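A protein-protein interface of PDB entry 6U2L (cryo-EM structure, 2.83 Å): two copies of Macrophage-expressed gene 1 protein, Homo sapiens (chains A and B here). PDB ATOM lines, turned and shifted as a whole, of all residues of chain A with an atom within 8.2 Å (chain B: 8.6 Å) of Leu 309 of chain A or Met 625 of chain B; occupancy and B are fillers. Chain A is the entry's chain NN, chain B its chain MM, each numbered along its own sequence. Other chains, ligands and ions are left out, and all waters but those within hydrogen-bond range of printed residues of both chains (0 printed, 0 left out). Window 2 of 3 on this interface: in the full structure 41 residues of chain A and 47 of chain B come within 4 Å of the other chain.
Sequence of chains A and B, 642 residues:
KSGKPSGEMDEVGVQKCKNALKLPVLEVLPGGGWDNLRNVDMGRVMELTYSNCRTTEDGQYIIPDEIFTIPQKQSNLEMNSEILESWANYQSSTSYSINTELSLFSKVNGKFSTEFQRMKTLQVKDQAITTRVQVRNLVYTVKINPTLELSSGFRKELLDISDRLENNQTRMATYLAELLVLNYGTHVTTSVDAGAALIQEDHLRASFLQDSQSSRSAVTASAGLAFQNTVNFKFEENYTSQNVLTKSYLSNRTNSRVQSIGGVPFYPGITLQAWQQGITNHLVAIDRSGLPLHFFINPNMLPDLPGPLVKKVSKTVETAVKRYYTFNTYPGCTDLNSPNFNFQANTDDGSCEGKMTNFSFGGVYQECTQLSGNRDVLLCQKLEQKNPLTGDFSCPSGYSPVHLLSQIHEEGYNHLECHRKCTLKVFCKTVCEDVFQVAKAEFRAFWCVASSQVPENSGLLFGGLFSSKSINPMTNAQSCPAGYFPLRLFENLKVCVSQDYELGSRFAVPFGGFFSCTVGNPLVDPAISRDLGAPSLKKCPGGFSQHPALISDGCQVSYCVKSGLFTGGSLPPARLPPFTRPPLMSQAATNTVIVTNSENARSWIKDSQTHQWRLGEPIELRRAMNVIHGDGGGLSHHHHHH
The side-chain carboxylate (OE1) of Glu 166 of chain A is in salt-bridge range of the guanidinium group (NH1) of Arg 623 of chain B, 3.0 Å away.
The side-chain amide nitrogen (ND2) of Asn 167 of chain A sits close to the guanidinium group (NH2) of Arg 623 of chain B, at 3.0 Å.
The side-chain amide oxygen (OD1) of Asn 167 of chain A sits close to the backbone carbonyl oxygen (O) of Asp 163 of chain A (2.9 Å).
Met 625 of chain B touches Pro 306 of chain A.
Gln 587 of chain B touches Pro 308 of chain A.
Val 627 of chain B touches Pro 308 of chain A (CG2 to CG, 3.6 Å).
CD1 of Leu 309 of chain A touches SD of Met 625 of chain B, at 3.97 Å.
Asp 304 of chain A touches none of the printed residues of chain B.
Printed residues of chain B within 4 Å of Pro 306 of chain A: Met 625 (3.7 Å).
Gly 307 of chain A touches none of the printed residues of chain B.
Of chain B, only Gln 587 (3.3 Å) and Val 627 (3.6 Å) come within 4 Å of Pro 308 of chain A.
Leu 309 of chain A touches just one residue of chain B: Met 625 (3.97 Å).
No residue of chain B comes within 4 Å of Val 310 of chain A.
Ser 314 of chain A touches none of the printed residues of chain B.
Printed residues of chain A within 4 Å of Gln 587 of chain B: Pro 308.
Of the printed residues of chain A, Arg 623 of chain B touches Glu 166 and Asn 167.
No residue of chain A comes within 4 Å of Ala 624 of chain B.
Met 625 of chain B touches two residues of chain A.
Printed residues of chain A within 4 Å of Val 627 of chain B: Pro 308.
The nearest residue of chain A that does not touch Met 625 of chain B is Pro 308 of chain A (4.1 Å).
The nearest printed residue of chain A that does not touch Gln 587 of chain B is Lys 312 of chain A (5.3 Å).
Of the 14 printed residues of chain B, 4 touch a printed residue of chain A.
Of the 25 printed residues of chain A, 5 touch a printed residue of chain B.
Hydrophobic or aromatic side chains of chain A that line the printed part of chain B: Pro 306, Pro 308 and Leu 309.
No position is printed for both chains.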
ATOM      1  N   LEU A 158      -1.703  10.652 -16.371  1.00  0.00           N
ATOM      2  CA  LEU A 158      -3.140  10.718 -16.146  1.00  0.00           C
ATOM      3  C   LEU A 158      -3.757  11.922 -16.827  1.00  0.00           C
ATOM      4  O   LEU A 158      -4.926  11.879 -17.207  1.00  0.00           O
ATOM      5  CB  LEU A 158      -3.465  10.792 -14.659  1.00  0.00           C
ATOM      6  CG  LEU A 158      -3.215   9.630 -13.719  1.00  0.00           C
ATOM      7  CD1 LEU A 158      -3.559  10.100 -12.339  1.00  0.00           C
ATOM      8  CD2 LEU A 158      -4.070   8.465 -14.104  1.00  0.00           C
ATOM      9  N   LEU A 159      -3.002  13.010 -16.952  1.00  0.00           N
ATOM     10  CA  LEU A 159      -3.481  14.183 -17.668  1.00  0.00           C
ATOM     11  C   LEU A 159      -3.514  13.967 -19.169  1.00  0.00           C
ATOM     12  O   LEU A 159      -4.295  14.623 -19.860  1.00  0.00           O
ATOM     13  CB  LEU A 159      -2.614  15.386 -17.314  1.00  0.00           C
ATOM     14  CG  LEU A 159      -3.094  16.323 -16.203  1.00  0.00           C
ATOM     15  CD1 LEU A 159      -3.266  15.667 -14.867  1.00  0.00           C
ATOM     16  CD2 LEU A 159      -2.097  17.452 -16.075  1.00  0.00           C
ATOM     17  N   ILE A 161      -4.327  10.952 -20.502  1.00  0.00           N
ATOM     18  CA  ILE A 161      -5.590  10.235 -20.631  1.00  0.00           C
ATOM     19  C   ILE A 161      -6.745  11.207 -20.486  1.00  0.00           C
ATOM     20  O   ILE A 161      -7.763  11.096 -21.174  1.00  0.00           O
ATOM     21  CB  ILE A 161      -5.663   9.111 -19.583  1.00  0.00           C
ATOM     22  CG1 ILE A 161      -4.503   8.145 -19.756  1.00  0.00           C
ATOM     23  CG2 ILE A 161      -6.959   8.339 -19.686  1.00  0.00           C
ATOM     24  CD1 ILE A 161      -4.341   7.214 -18.601  1.00  0.00           C
ATOM     25  N   SER A 162      -6.581  12.195 -19.608  1.00  0.00           N
ATOM     26  CA  SER A 162      -7.614  13.190 -19.349  1.00  0.00           C
ATOM     27  C   SER A 162      -7.921  14.033 -20.578  1.00  0.00           C
ATOM     28  O   SER A 162      -9.074  14.409 -20.802  1.00  0.00           O
ATOM     29  CB  SER A 162      -7.167  14.076 -18.197  1.00  0.00           C
ATOM     30  OG  SER A 162      -8.016  15.183 -18.055  1.00  0.00           O
ATOM     31  N   ASP A 163      -6.904  14.332 -21.388  1.00  0.00           N
ATOM     32  CA  ASP A 163      -7.119  15.136 -22.587  1.00  0.00           C
ATOM     33  C   ASP A 163      -7.914  14.377 -23.632  1.00  0.00           C
ATOM     34  O   ASP A 163      -8.731  14.967 -24.343  1.00  0.00           O
ATOM     35  CB  ASP A 163      -5.783  15.576 -23.174  1.00  0.00           C
ATOM     36  CG  ASP A 163      -5.079  16.597 -22.321  1.00  0.00           C
ATOM     37  OD1 ASP A 163      -5.763  17.343 -21.593  1.00  0.00           O
ATOM     38  OD2 ASP A 163      -3.837  16.663 -22.387  1.00  0.00           O
ATOM     39  N   ARG A 164      -7.693  13.070 -23.738  1.00  0.00           N
ATOM     40  CA  ARG A 164      -8.390  12.267 -24.731  1.00  0.00           C
ATOM     41  C   ARG A 164      -9.851  12.052 -24.369  1.00  0.00           C
ATOM     42  O   ARG A 164     -10.683  11.884 -25.260  1.00  0.00           O
ATOM     43  CB  ARG A 164      -7.687  10.927 -24.885  1.00  0.00           C
ATOM     44  CG  ARG A 164      -6.238  11.021 -25.274  1.00  0.00           C
ATOM     45  CD  ARG A 164      -6.097  11.421 -26.701  1.00  0.00           C
ATOM     46  NE  ARG A 164      -4.710  11.423 -27.141  1.00  0.00           N
ATOM     47  CZ  ARG A 164      -4.323  11.757 -28.366  1.00  0.00           C
ATOM     48  NH1 ARG A 164      -5.223  12.111 -29.271  1.00  0.00           N
ATOM     49  NH2 ARG A 164      -3.042  11.734 -28.690  1.00  0.00           N
ATOM     50  N   LEU A 165     -10.188  12.036 -23.079  1.00  0.00           N
ATOM     51  CA  LEU A 165     -11.592  11.937 -22.699  1.00  0.00           C
ATOM     52  C   LEU A 165     -12.351  13.229 -22.947  1.00  0.00           C
ATOM     53  O   LEU A 165     -13.578  13.193 -23.094  1.00  0.00           O
ATOM     54  CB  LEU A 165     -11.751  11.563 -21.226  1.00  0.00           C
ATOM     55  CG  LEU A 165     -11.820  10.112 -20.740  1.00  0.00           C
ATOM     56  CD1 LEU A 165     -12.905   9.346 -21.477  1.00  0.00           C
ATOM     57  CD2 LEU A 165     -10.517   9.394 -20.805  1.00  0.00           C
ATOM     58  N   GLU A 166     -11.657  14.366 -22.970  1.00  0.00           N
ATOM     59  CA  GLU A 166     -12.302  15.634 -23.287  1.00  0.00           C
ATOM     60  C   GLU A 166     -12.715  15.688 -24.749  1.00  0.00           C
ATOM     61  O   GLU A 166     -13.839  16.080 -25.076  1.00  0.00           O
ATOM     62  CB  GLU A 166     -11.352  16.785 -22.977  1.00  0.00           C
ATOM     63  CG  GLU A 166     -11.008  16.939 -21.530  1.00  0.00           C
ATOM     64  CD  GLU A 166      -9.994  18.039 -21.303  1.00  0.00           C
ATOM     65  OE1 GLU A 166      -9.564  18.675 -22.285  1.00  0.00           O
ATOM     66  OE2 GLU A 166      -9.591  18.242 -20.142  1.00  0.00           O
ATOM     67  N   ASN A 167     -11.821  15.275 -25.638  1.00  0.00           N
ATOM     68  CA  ASN A 167     -11.988  15.374 -27.075  1.00  0.00           C
ATOM     69  C   ASN A 167     -12.836  14.267 -27.668  1.00  0.00           C
ATOM     70  O   ASN A 167     -12.896  14.189 -28.899  1.00  0.00           O
ATOM     71  CB  ASN A 167     -10.620  15.368 -27.752  1.00  0.00           C
ATOM     72  CG  ASN A 167      -9.818  16.600 -27.441  1.00  0.00           C
ATOM     73  OD1 ASN A 167      -8.795  16.542 -26.771  1.00  0.00           O
ATOM     74  ND2 ASN A 167     -10.273  17.733 -27.944  1.00  0.00           N
ATOM     75  N   ILE A 297      -7.129   7.550  -7.986  1.00  0.00           N
ATOM     76  CA  ILE A 297      -7.594   8.491  -8.990  1.00  0.00           C
ATOM     77  C   ILE A 297      -8.949   8.996  -8.520  1.00  0.00           C
ATOM     78  O   ILE A 297      -9.988   8.394  -8.796  1.00  0.00           O
ATOM     79  CB  ILE A 297      -7.668   7.840 -10.379  1.00  0.00           C
ATOM     80  CG1 ILE A 297      -6.313   7.251 -10.739  1.00  0.00           C
ATOM     81  CG2 ILE A 297      -8.021   8.868 -11.418  1.00  0.00           C
ATOM     82  CD1 ILE A 297      -6.359   6.354 -11.926  1.00  0.00           C
ATOM     83  N   PRO A 299     -11.049  12.908  -6.911  1.00  0.00           N
ATOM     84  CA  PRO A 299     -10.932  14.378  -6.949  1.00  0.00           C
ATOM     85  C   PRO A 299      -9.999  14.987  -5.917  1.00  0.00           C
ATOM     86  O   PRO A 299      -9.642  16.160  -6.060  1.00  0.00           O
ATOM     87  CB  PRO A 299     -12.369  14.850  -6.723  1.00  0.00           C
ATOM     88  CG  PRO A 299     -13.183  13.778  -7.229  1.00  0.00           C
ATOM     89  CD  PRO A 299     -12.473  12.516  -6.913  1.00  0.00           C
ATOM     90  N   LEU A 302      -6.333  14.813  -7.603  1.00  0.00           N
ATOM     91  CA  LEU A 302      -6.292  15.631  -8.811  1.00  0.00           C
ATOM     92  C   LEU A 302      -7.172  16.851  -8.576  1.00  0.00           C
ATOM     93  O   LEU A 302      -8.350  16.862  -8.963  1.00  0.00           O
ATOM     94  CB  LEU A 302      -6.755  14.826 -10.021  1.00  0.00           C
ATOM     95  CG  LEU A 302      -5.864  13.642 -10.387  1.00  0.00           C
ATOM     96  CD1 LEU A 302      -6.545  12.772 -11.402  1.00  0.00           C
ATOM     97  CD2 LEU A 302      -4.544  14.136 -10.932  1.00  0.00           C
ATOM     98  N   ASP A 304      -6.784  19.939  -9.772  1.00  0.00           N
ATOM     99  CA  ASP A 304      -6.796  20.867 -10.891  1.00  0.00           C
ATOM    100  C   ASP A 304      -7.589  20.339 -12.080  1.00  0.00           C
ATOM    101  O   ASP A 304      -7.381  20.798 -13.208  1.00  0.00           O
ATOM    102  CB  ASP A 304      -5.367  21.198 -11.314  1.00  0.00           C
ATOM    103  CG  ASP A 304      -4.664  22.102 -10.324  1.00  0.00           C
ATOM    104  OD1 ASP A 304      -5.350  22.899  -9.654  1.00  0.00           O
ATOM    105  OD2 ASP A 304      -3.422  22.024 -10.223  1.00  0.00           O
ATOM    106  N   LEU A 305      -8.484  19.387 -11.856  1.00  0.00           N
ATOM    107  CA  LEU A 305      -9.362  18.851 -12.879  1.00  0.00           C
ATOM    108  C   LEU A 305     -10.777  18.795 -12.331  1.00  0.00           C
ATOM    109  O   LEU A 305     -10.961  18.724 -11.115  1.00  0.00           O
ATOM    110  CB  LEU A 305      -8.918  17.452 -13.321  1.00  0.00           C
ATOM    111  CG  LEU A 305      -7.619  17.382 -14.104  1.00  0.00           C
ATOM    112  CD1 LEU A 305      -7.294  15.948 -14.414  1.00  0.00           C
ATOM    113  CD2 LEU A 305      -7.735  18.190 -15.370  1.00  0.00           C
ATOM    114  N   PRO A 306     -11.792  18.854 -13.189  1.00  0.00           N
ATOM    115  CA  PRO A 306     -13.167  18.786 -12.695  1.00  0.00           C
ATOM    116  C   PRO A 306     -13.527  17.418 -12.142  1.00  0.00           C
ATOM    117  O   PRO A 306     -12.863  16.417 -12.390  1.00  0.00           O
ATOM    118  CB  PRO A 306     -14.004  19.129 -13.930  1.00  0.00           C
ATOM    119  CG  PRO A 306     -13.134  18.909 -15.060  1.00  0.00           C
ATOM    120  CD  PRO A 306     -11.762  19.222 -14.612  1.00  0.00           C
ATOM    121  N   GLY A 307     -14.602  17.412 -11.362  1.00  0.00           N
ATOM    122  CA  GLY A 307     -15.092  16.249 -10.661  1.00  0.00           C
ATOM    123  C   GLY A 307     -15.466  15.050 -11.509  1.00  0.00           C
ATOM    124  O   GLY A 307     -14.928  13.961 -11.315  1.00  0.00           O
ATOM    125  N   PRO A 308     -16.409  15.201 -12.447  1.00  0.00           N
ATOM    126  CA  PRO A 308     -16.785  14.053 -13.284  1.00  0.00           C
ATOM    127  C   PRO A 308     -15.742  13.641 -14.286  1.00  0.00           C
ATOM    128  O   PRO A 308     -15.898  12.580 -14.894  1.00  0.00           O
ATOM    129  CB  PRO A 308     -18.039  14.539 -14.006  1.00  0.00           C
ATOM    130  CG  PRO A 308     -18.567  15.569 -13.159  1.00  0.00           C
ATOM    131  CD  PRO A 308     -17.403  16.276 -12.569  1.00  0.00           C
ATOM    132  N   LEU A 309     -14.712  14.441 -14.503  1.00  0.00           N
ATOM    133  CA  LEU A 309     -13.690  14.099 -15.472  1.00  0.00           C
ATOM    134  C   LEU A 309     -12.581  13.244 -14.879  1.00  0.00           C
ATOM    135  O   LEU A 309     -11.936  12.491 -15.613  1.00  0.00           O
ATOM    136  CB  LEU A 309     -13.144  15.384 -16.085  1.00  0.00           C
ATOM    137  CG  LEU A 309     -12.077  15.420 -17.162  1.00  0.00           C
ATOM    138  CD1 LEU A 309     -12.432  16.504 -18.119  1.00  0.00           C
ATOM    139  CD2 LEU A 309     -10.792  15.784 -16.499  1.00  0.00           C
ATOM    140  N   VAL A 310     -12.348  13.320 -13.568  1.00  0.00           N
ATOM    141  CA  VAL A 310     -11.421  12.380 -12.943  1.00  0.00           C
ATOM    142  C   VAL A 310     -12.091  11.062 -12.615  1.00  0.00           C
ATOM    143  O   VAL A 310     -11.405  10.118 -12.218  1.00  0.00           O
ATOM    144  CB  VAL A 310     -10.791  12.916 -11.647  1.00  0.00           C
ATOM    145  CG1 VAL A 310     -10.063  14.202 -11.912  1.00  0.00           C
ATOM    146  CG2 VAL A 310     -11.833  13.110 -10.601  1.00  0.00           C
ATOM    147  N   LYS A 311     -13.408  10.978 -12.753  1.00  0.00           N
ATOM    148  CA  LYS A 311     -14.116   9.714 -12.668  1.00  0.00           C
ATOM    149  C   LYS A 311     -14.186   8.998 -14.004  1.00  0.00           C
ATOM    150  O   LYS A 311     -14.505   7.809 -14.036  1.00  0.00           O
ATOM    151  CB  LYS A 311     -15.530   9.943 -12.145  1.00  0.00           C
ATOM    152  CG  LYS A 311     -15.574  10.467 -10.738  1.00  0.00           C
ATOM    153  CD  LYS A 311     -16.998  10.662 -10.283  1.00  0.00           C
ATOM    154  CE  LYS A 311     -17.053  11.261  -8.893  1.00  0.00           C
ATOM    155  NZ  LYS A 311     -16.571  10.302  -7.867  1.00  0.00           N
ATOM    156  N   LYS A 312     -13.925   9.696 -15.105  1.00  0.00           N
ATOM    157  CA  LYS A 312     -13.762   9.020 -16.382  1.00  0.00           C
ATOM    158  C   LYS A 312     -12.375   8.414 -16.491  1.00  0.00           C
ATOM    159  O   LYS A 312     -12.202   7.352 -17.094  1.00  0.00           O
ATOM    160  CB  LYS A 312     -13.990   9.995 -17.534  1.00  0.00           C
ATOM    161  CG  LYS A 312     -15.350  10.638 -17.564  1.00  0.00           C
ATOM    162  CD  LYS A 312     -16.417   9.677 -18.007  1.00  0.00           C
ATOM    163  CE  LYS A 312     -17.780  10.344 -17.957  1.00  0.00           C
ATOM    164  NZ  LYS A 312     -17.894  11.456 -18.938  1.00  0.00           N
ATOM    165  N   VAL A 313     -11.377   9.096 -15.931  1.00  0.00           N
ATOM    166  CA  VAL A 313     -10.019   8.570 -15.909  1.00  0.00           C
ATOM    167  C   VAL A 313      -9.936   7.372 -14.978  1.00  0.00           C
ATOM    168  O   VAL A 313      -9.274   6.377 -15.279  1.00  0.00           O
ATOM    169  CB  VAL A 313      -9.040   9.683 -15.500  1.00  0.00           C
ATOM    170  CG1 VAL A 313      -7.623   9.176 -15.444  1.00  0.00           C
ATOM    171  CG2 VAL A 313      -9.140  10.841 -16.448  1.00  0.00           C
ATOM    172  N   SER A 314     -10.633   7.438 -13.846  1.00  0.00           N
ATOM    173  CA  SER A 314     -10.617   6.344 -12.887  1.00  0.00           C
ATOM    174  C   SER A 314     -11.354   5.124 -13.408  1.00  0.00           C
ATOM    175  O   SER A 314     -11.013   3.997 -13.047  1.00  0.00           O
ATOM    176  CB  SER A 314     -11.231   6.804 -11.574  1.00  0.00           C
ATOM    177  OG  SER A 314     -11.274   5.748 -10.642  1.00  0.00           O
ATOM    178  N   LYS A 315     -12.354   5.322 -14.256  1.00  0.00           N
ATOM    179  CA  LYS A 315     -13.093   4.193 -14.794  1.00  0.00           C
ATOM    180  C   LYS A 315     -12.384   3.578 -15.990  1.00  0.00           C
ATOM    181  O   LYS A 315     -12.467   2.366 -16.197  1.00  0.00           O
ATOM    182  CB  LYS A 315     -14.505   4.638 -15.164  1.00  0.00           C
ATOM    183  CG  LYS A 315     -15.409   3.536 -15.640  1.00  0.00           C
ATOM    184  CD  LYS A 315     -15.682   2.564 -14.521  1.00  0.00           C
ATOM    185  CE  LYS A 315     -16.640   1.478 -14.959  1.00  0.00           C
ATOM    186  NZ  LYS A 315     -16.856   0.475 -13.884  1.00  0.00           N
ATOM    187  N   THR A 316     -11.658   4.371 -16.769  1.00  0.00           N
ATOM    188  CA  THR A 316     -10.951   3.800 -17.903  1.00  0.00           C
ATOM    189  C   THR A 316      -9.651   3.113 -17.503  1.00  0.00           C
ATOM    190  O   THR A 316      -9.088   2.379 -18.317  1.00  0.00           O
ATOM    191  CB  THR A 316     -10.681   4.872 -18.962  1.00  0.00           C
ATOM    192  OG1 THR A 316     -10.267   4.243 -20.175  1.00  0.00           O
ATOM    193  CG2 THR A 316      -9.589   5.792 -18.528  1.00  0.00           C
ATOM    194  N   ASP B 434     -24.293  18.418 -23.787  1.00  0.00           N
ATOM    195  CA  ASP B 434     -24.413  17.004 -23.430  1.00  0.00           C
ATOM    196  C   ASP B 434     -24.873  16.891 -21.981  1.00  0.00           C
ATOM    197  O   ASP B 434     -24.072  17.051 -21.060  1.00  0.00           O
ATOM    198  CB  ASP B 434     -23.090  16.284 -23.636  1.00  0.00           C
ATOM    199  CG  ASP B 434     -23.184  14.802 -23.357  1.00  0.00           C
ATOM    200  OD1 ASP B 434     -23.709  14.059 -24.211  1.00  0.00           O
ATOM    201  OD2 ASP B 434     -22.736  14.377 -22.275  1.00  0.00           O
ATOM    202  N   SER B 586     -26.352  14.603 -11.454  1.00  0.00           N
ATOM    203  CA  SER B 586     -26.739  15.063 -12.776  1.00  0.00           C
ATOM    204  C   SER B 586     -25.815  16.180 -13.245  1.00  0.00           C
ATOM    205  O   SER B 586     -25.479  17.089 -12.486  1.00  0.00           O
ATOM    206  CB  SER B 586     -28.199  15.508 -12.780  1.00  0.00           C
ATOM    207  OG  SER B 586     -28.434  16.525 -11.838  1.00  0.00           O
ATOM    208  N   GLN B 587     -25.394  16.091 -14.504  1.00  0.00           N
ATOM    209  CA  GLN B 587     -24.271  16.843 -15.042  1.00  0.00           C
ATOM    210  C   GLN B 587     -24.690  17.542 -16.326  1.00  0.00           C
ATOM    211  O   GLN B 587     -25.796  17.348 -16.830  1.00  0.00           O
ATOM    212  CB  GLN B 587     -23.085  15.915 -15.314  1.00  0.00           C
ATOM    213  CG  GLN B 587     -22.558  15.227 -14.086  1.00  0.00           C
ATOM    214  CD  GLN B 587     -21.554  14.156 -14.412  1.00  0.00           C
ATOM    215  OE1 GLN B 587     -21.246  13.909 -15.574  1.00  0.00           O
ATOM    216  NE2 GLN B 587     -21.061  13.479 -13.385  1.00  0.00           N
ATOM    217  N   ALA B 588     -23.780  18.352 -16.863  1.00  0.00           N
ATOM    218  CA  ALA B 588     -23.971  19.047 -18.129  1.00  0.00           C
ATOM    219  C   ALA B 588     -22.607  19.462 -18.653  1.00  0.00           C
ATOM    220  O   ALA B 588     -21.753  19.891 -17.880  1.00  0.00           O
ATOM    221  CB  ALA B 588     -24.868  20.277 -17.977  1.00  0.00           C
ATOM    222  N   ALA B 589     -22.406  19.328 -19.958  1.00  0.00           N
ATOM    223  CA  ALA B 589     -21.125  19.657 -20.563  1.00  0.00           C
ATOM    224  C   ALA B 589     -21.358  20.296 -21.919  1.00  0.00           C
ATOM    225  O   ALA B 589     -22.032  19.713 -22.770  1.00  0.00           O
ATOM    226  CB  ALA B 589     -20.249  18.413 -20.712  1.00  0.00           C
ATOM    227  N   THR B 590     -20.794  21.485 -22.122  1.00  0.00           N
ATOM    228  CA  THR B 590     -20.957  22.231 -23.359  1.00  0.00           C
ATOM    229  C   THR B 590     -19.609  22.440 -24.030  1.00  0.00           C
ATOM    230  O   THR B 590     -18.561  22.399 -23.386  1.00  0.00           O
ATOM    231  CB  THR B 590     -21.612  23.590 -23.113  1.00  0.00           C
ATOM    232  OG1 THR B 590     -20.740  24.399 -22.319  1.00  0.00           O
ATOM    233  CG2 THR B 590     -22.930  23.426 -22.378  1.00  0.00           C
ATOM    234  N   ASN B 591     -19.655  22.674 -25.342  1.00  0.00           N
ATOM    235  CA  ASN B 591     -18.467  22.882 -26.173  1.00  0.00           C
ATOM    236  C   ASN B 591     -18.838  23.904 -27.240  1.00  0.00           C
ATOM    237  O   ASN B 591     -19.465  23.544 -28.238  1.00  0.00           O
ATOM    238  CB  ASN B 591     -18.008  21.589 -26.834  1.00  0.00           C
ATOM    239  CG  ASN B 591     -17.464  20.585 -25.858  1.00  0.00           C
ATOM    240  OD1 ASN B 591     -16.695  20.918 -24.968  1.00  0.00           O
ATOM    241  ND2 ASN B 591     -17.858  19.331 -26.028  1.00  0.00           N
ATOM    242  N   ARG B 622     -14.149  27.043 -26.223  1.00  0.00           N
ATOM    243  CA  ARG B 622     -14.498  27.142 -24.810  1.00  0.00           C
ATOM    244  C   ARG B 622     -15.122  25.831 -24.331  1.00  0.00           C
ATOM    245  O   ARG B 622     -15.754  25.107 -25.102  1.00  0.00           O
ATOM    246  CB  ARG B 622     -15.472  28.305 -24.601  1.00  0.00           C
ATOM    247  CG  ARG B 622     -15.834  28.648 -23.170  1.00  0.00           C
ATOM    248  CD  ARG B 622     -16.832  29.771 -23.133  1.00  0.00           C
ATOM    249  NE  ARG B 622     -17.367  30.011 -21.796  1.00  0.00           N
ATOM    250  CZ  ARG B 622     -16.858  30.868 -20.920  1.00  0.00           C
ATOM    251  NH1 ARG B 622     -15.793  31.592 -21.227  1.00  0.00           N
ATOM    252  NH2 ARG B 622     -17.430  31.014 -19.736  1.00  0.00           N
ATOM    253  N   ARG B 623     -14.922  25.508 -23.050  1.00  0.00           N
ATOM    254  CA  ARG B 623     -15.504  24.319 -22.432  1.00  0.00           C
ATOM    255  C   ARG B 623     -16.073  24.647 -21.064  1.00  0.00           C
ATOM    256  O   ARG B 623     -15.587  25.539 -20.373  1.00  0.00           O
ATOM    257  CB  ARG B 623     -14.477  23.204 -22.297  1.00  0.00           C
ATOM    258  CG  ARG B 623     -14.220  22.530 -23.590  1.00  0.00           C
ATOM    259  CD  ARG B 623     -13.103  21.555 -23.549  1.00  0.00           C
ATOM    260  NE  ARG B 623     -13.031  20.903 -24.845  1.00  0.00           N
ATOM    261  CZ  ARG B 623     -12.005  20.185 -25.267  1.00  0.00           C
ATOM    262  NH1 ARG B 623     -10.934  20.055 -24.505  1.00  0.00           N
ATOM    263  NH2 ARG B 623     -12.041  19.627 -26.465  1.00  0.00           N
ATOM    264  N   ALA B 624     -17.103  23.904 -20.673  1.00  0.00           N
ATOM    265  CA  ALA B 624     -17.723  24.083 -19.370  1.00  0.00           C
ATOM    266  C   ALA B 624     -18.317  22.766 -18.901  1.00  0.00           C
ATOM    267  O   ALA B 624     -18.870  22.013 -19.704  1.00  0.00           O
ATOM    268  CB  ALA B 624     -18.809  25.157 -19.409  1.00  0.00           C
ATOM    269  N   MET B 625     -18.191  22.488 -17.604  1.00  0.00           N
ATOM    270  CA  MET B 625     -18.800  21.314 -16.989  1.00  0.00           C
ATOM    271  C   MET B 625     -19.575  21.753 -15.759  1.00  0.00           C
ATOM    272  O   MET B 625     -18.997  22.320 -14.834  1.00  0.00           O
ATOM    273  CB  MET B 625     -17.751  20.263 -16.616  1.00  0.00           C
ATOM    274  CG  MET B 625     -17.062  19.652 -17.821  1.00  0.00           C
ATOM    275  SD  MET B 625     -15.887  18.338 -17.468  1.00  0.00           S
ATOM    276  CE  MET B 625     -17.009  17.006 -17.084  1.00  0.00           C
ATOM    277  N   ASN B 626     -20.874  21.478 -15.746  1.00  0.00           N
ATOM    278  CA  ASN B 626     -21.781  21.940 -14.704  1.00  0.00           C
ATOM    279  C   ASN B 626     -22.329  20.734 -13.957  1.00  0.00           C
ATOM    280  O   ASN B 626     -22.925  19.846 -14.568  1.00  0.00           O
ATOM    281  CB  ASN B 626     -22.927  22.739 -15.315  1.00  0.00           C
ATOM    282  CG  ASN B 626     -22.458  23.994 -15.995  1.00  0.00           C
ATOM    283  OD1 ASN B 626     -21.656  24.748 -15.453  1.00  0.00           O
ATOM    284  ND2 ASN B 626     -22.935  24.212 -17.208  1.00  0.00           N
ATOM    285  N   VAL B 627     -22.135  20.706 -12.643  1.00  0.00           N
ATOM    286  CA  VAL B 627     -22.575  19.606 -11.793  1.00  0.00           C
ATOM    287  C   VAL B 627     -23.525  20.179 -10.756  1.00  0.00           C
ATOM    288  O   VAL B 627     -23.276  21.266 -10.231  1.00  0.00           O
ATOM    289  CB  VAL B 627     -21.378  18.918 -11.102  1.00  0.00           C
ATOM    290  CG1 VAL B 627     -21.808  17.704 -10.313  1.00  0.00           C
ATOM    291  CG2 VAL B 627     -20.339  18.550 -12.097  1.00  0.00           C
ATOM    292  N   ILE B 628     -24.612  19.470 -10.466  1.00  0.00           N
ATOM    293  CA  ILE B 628     -25.492  19.808  -9.354  1.00  0.00           C
ATOM    294  C   ILE B 628     -25.632  18.596  -8.439  1.00  0.00           C
ATOM    295  O   ILE B 628     -25.892  17.482  -8.903  1.00  0.00           O
ATOM    296  CB  ILE B 628     -26.864  20.326  -9.840  1.00  0.00           C
ATOM    297  CG1 ILE B 628     -27.830  20.483  -8.667  1.00  0.00           C
ATOM    298  CG2 ILE B 628     -27.417  19.508 -10.969  1.00  0.00           C
ATOM    299  CD1 ILE B 628     -29.110  21.135  -9.015  1.00  0.00           C
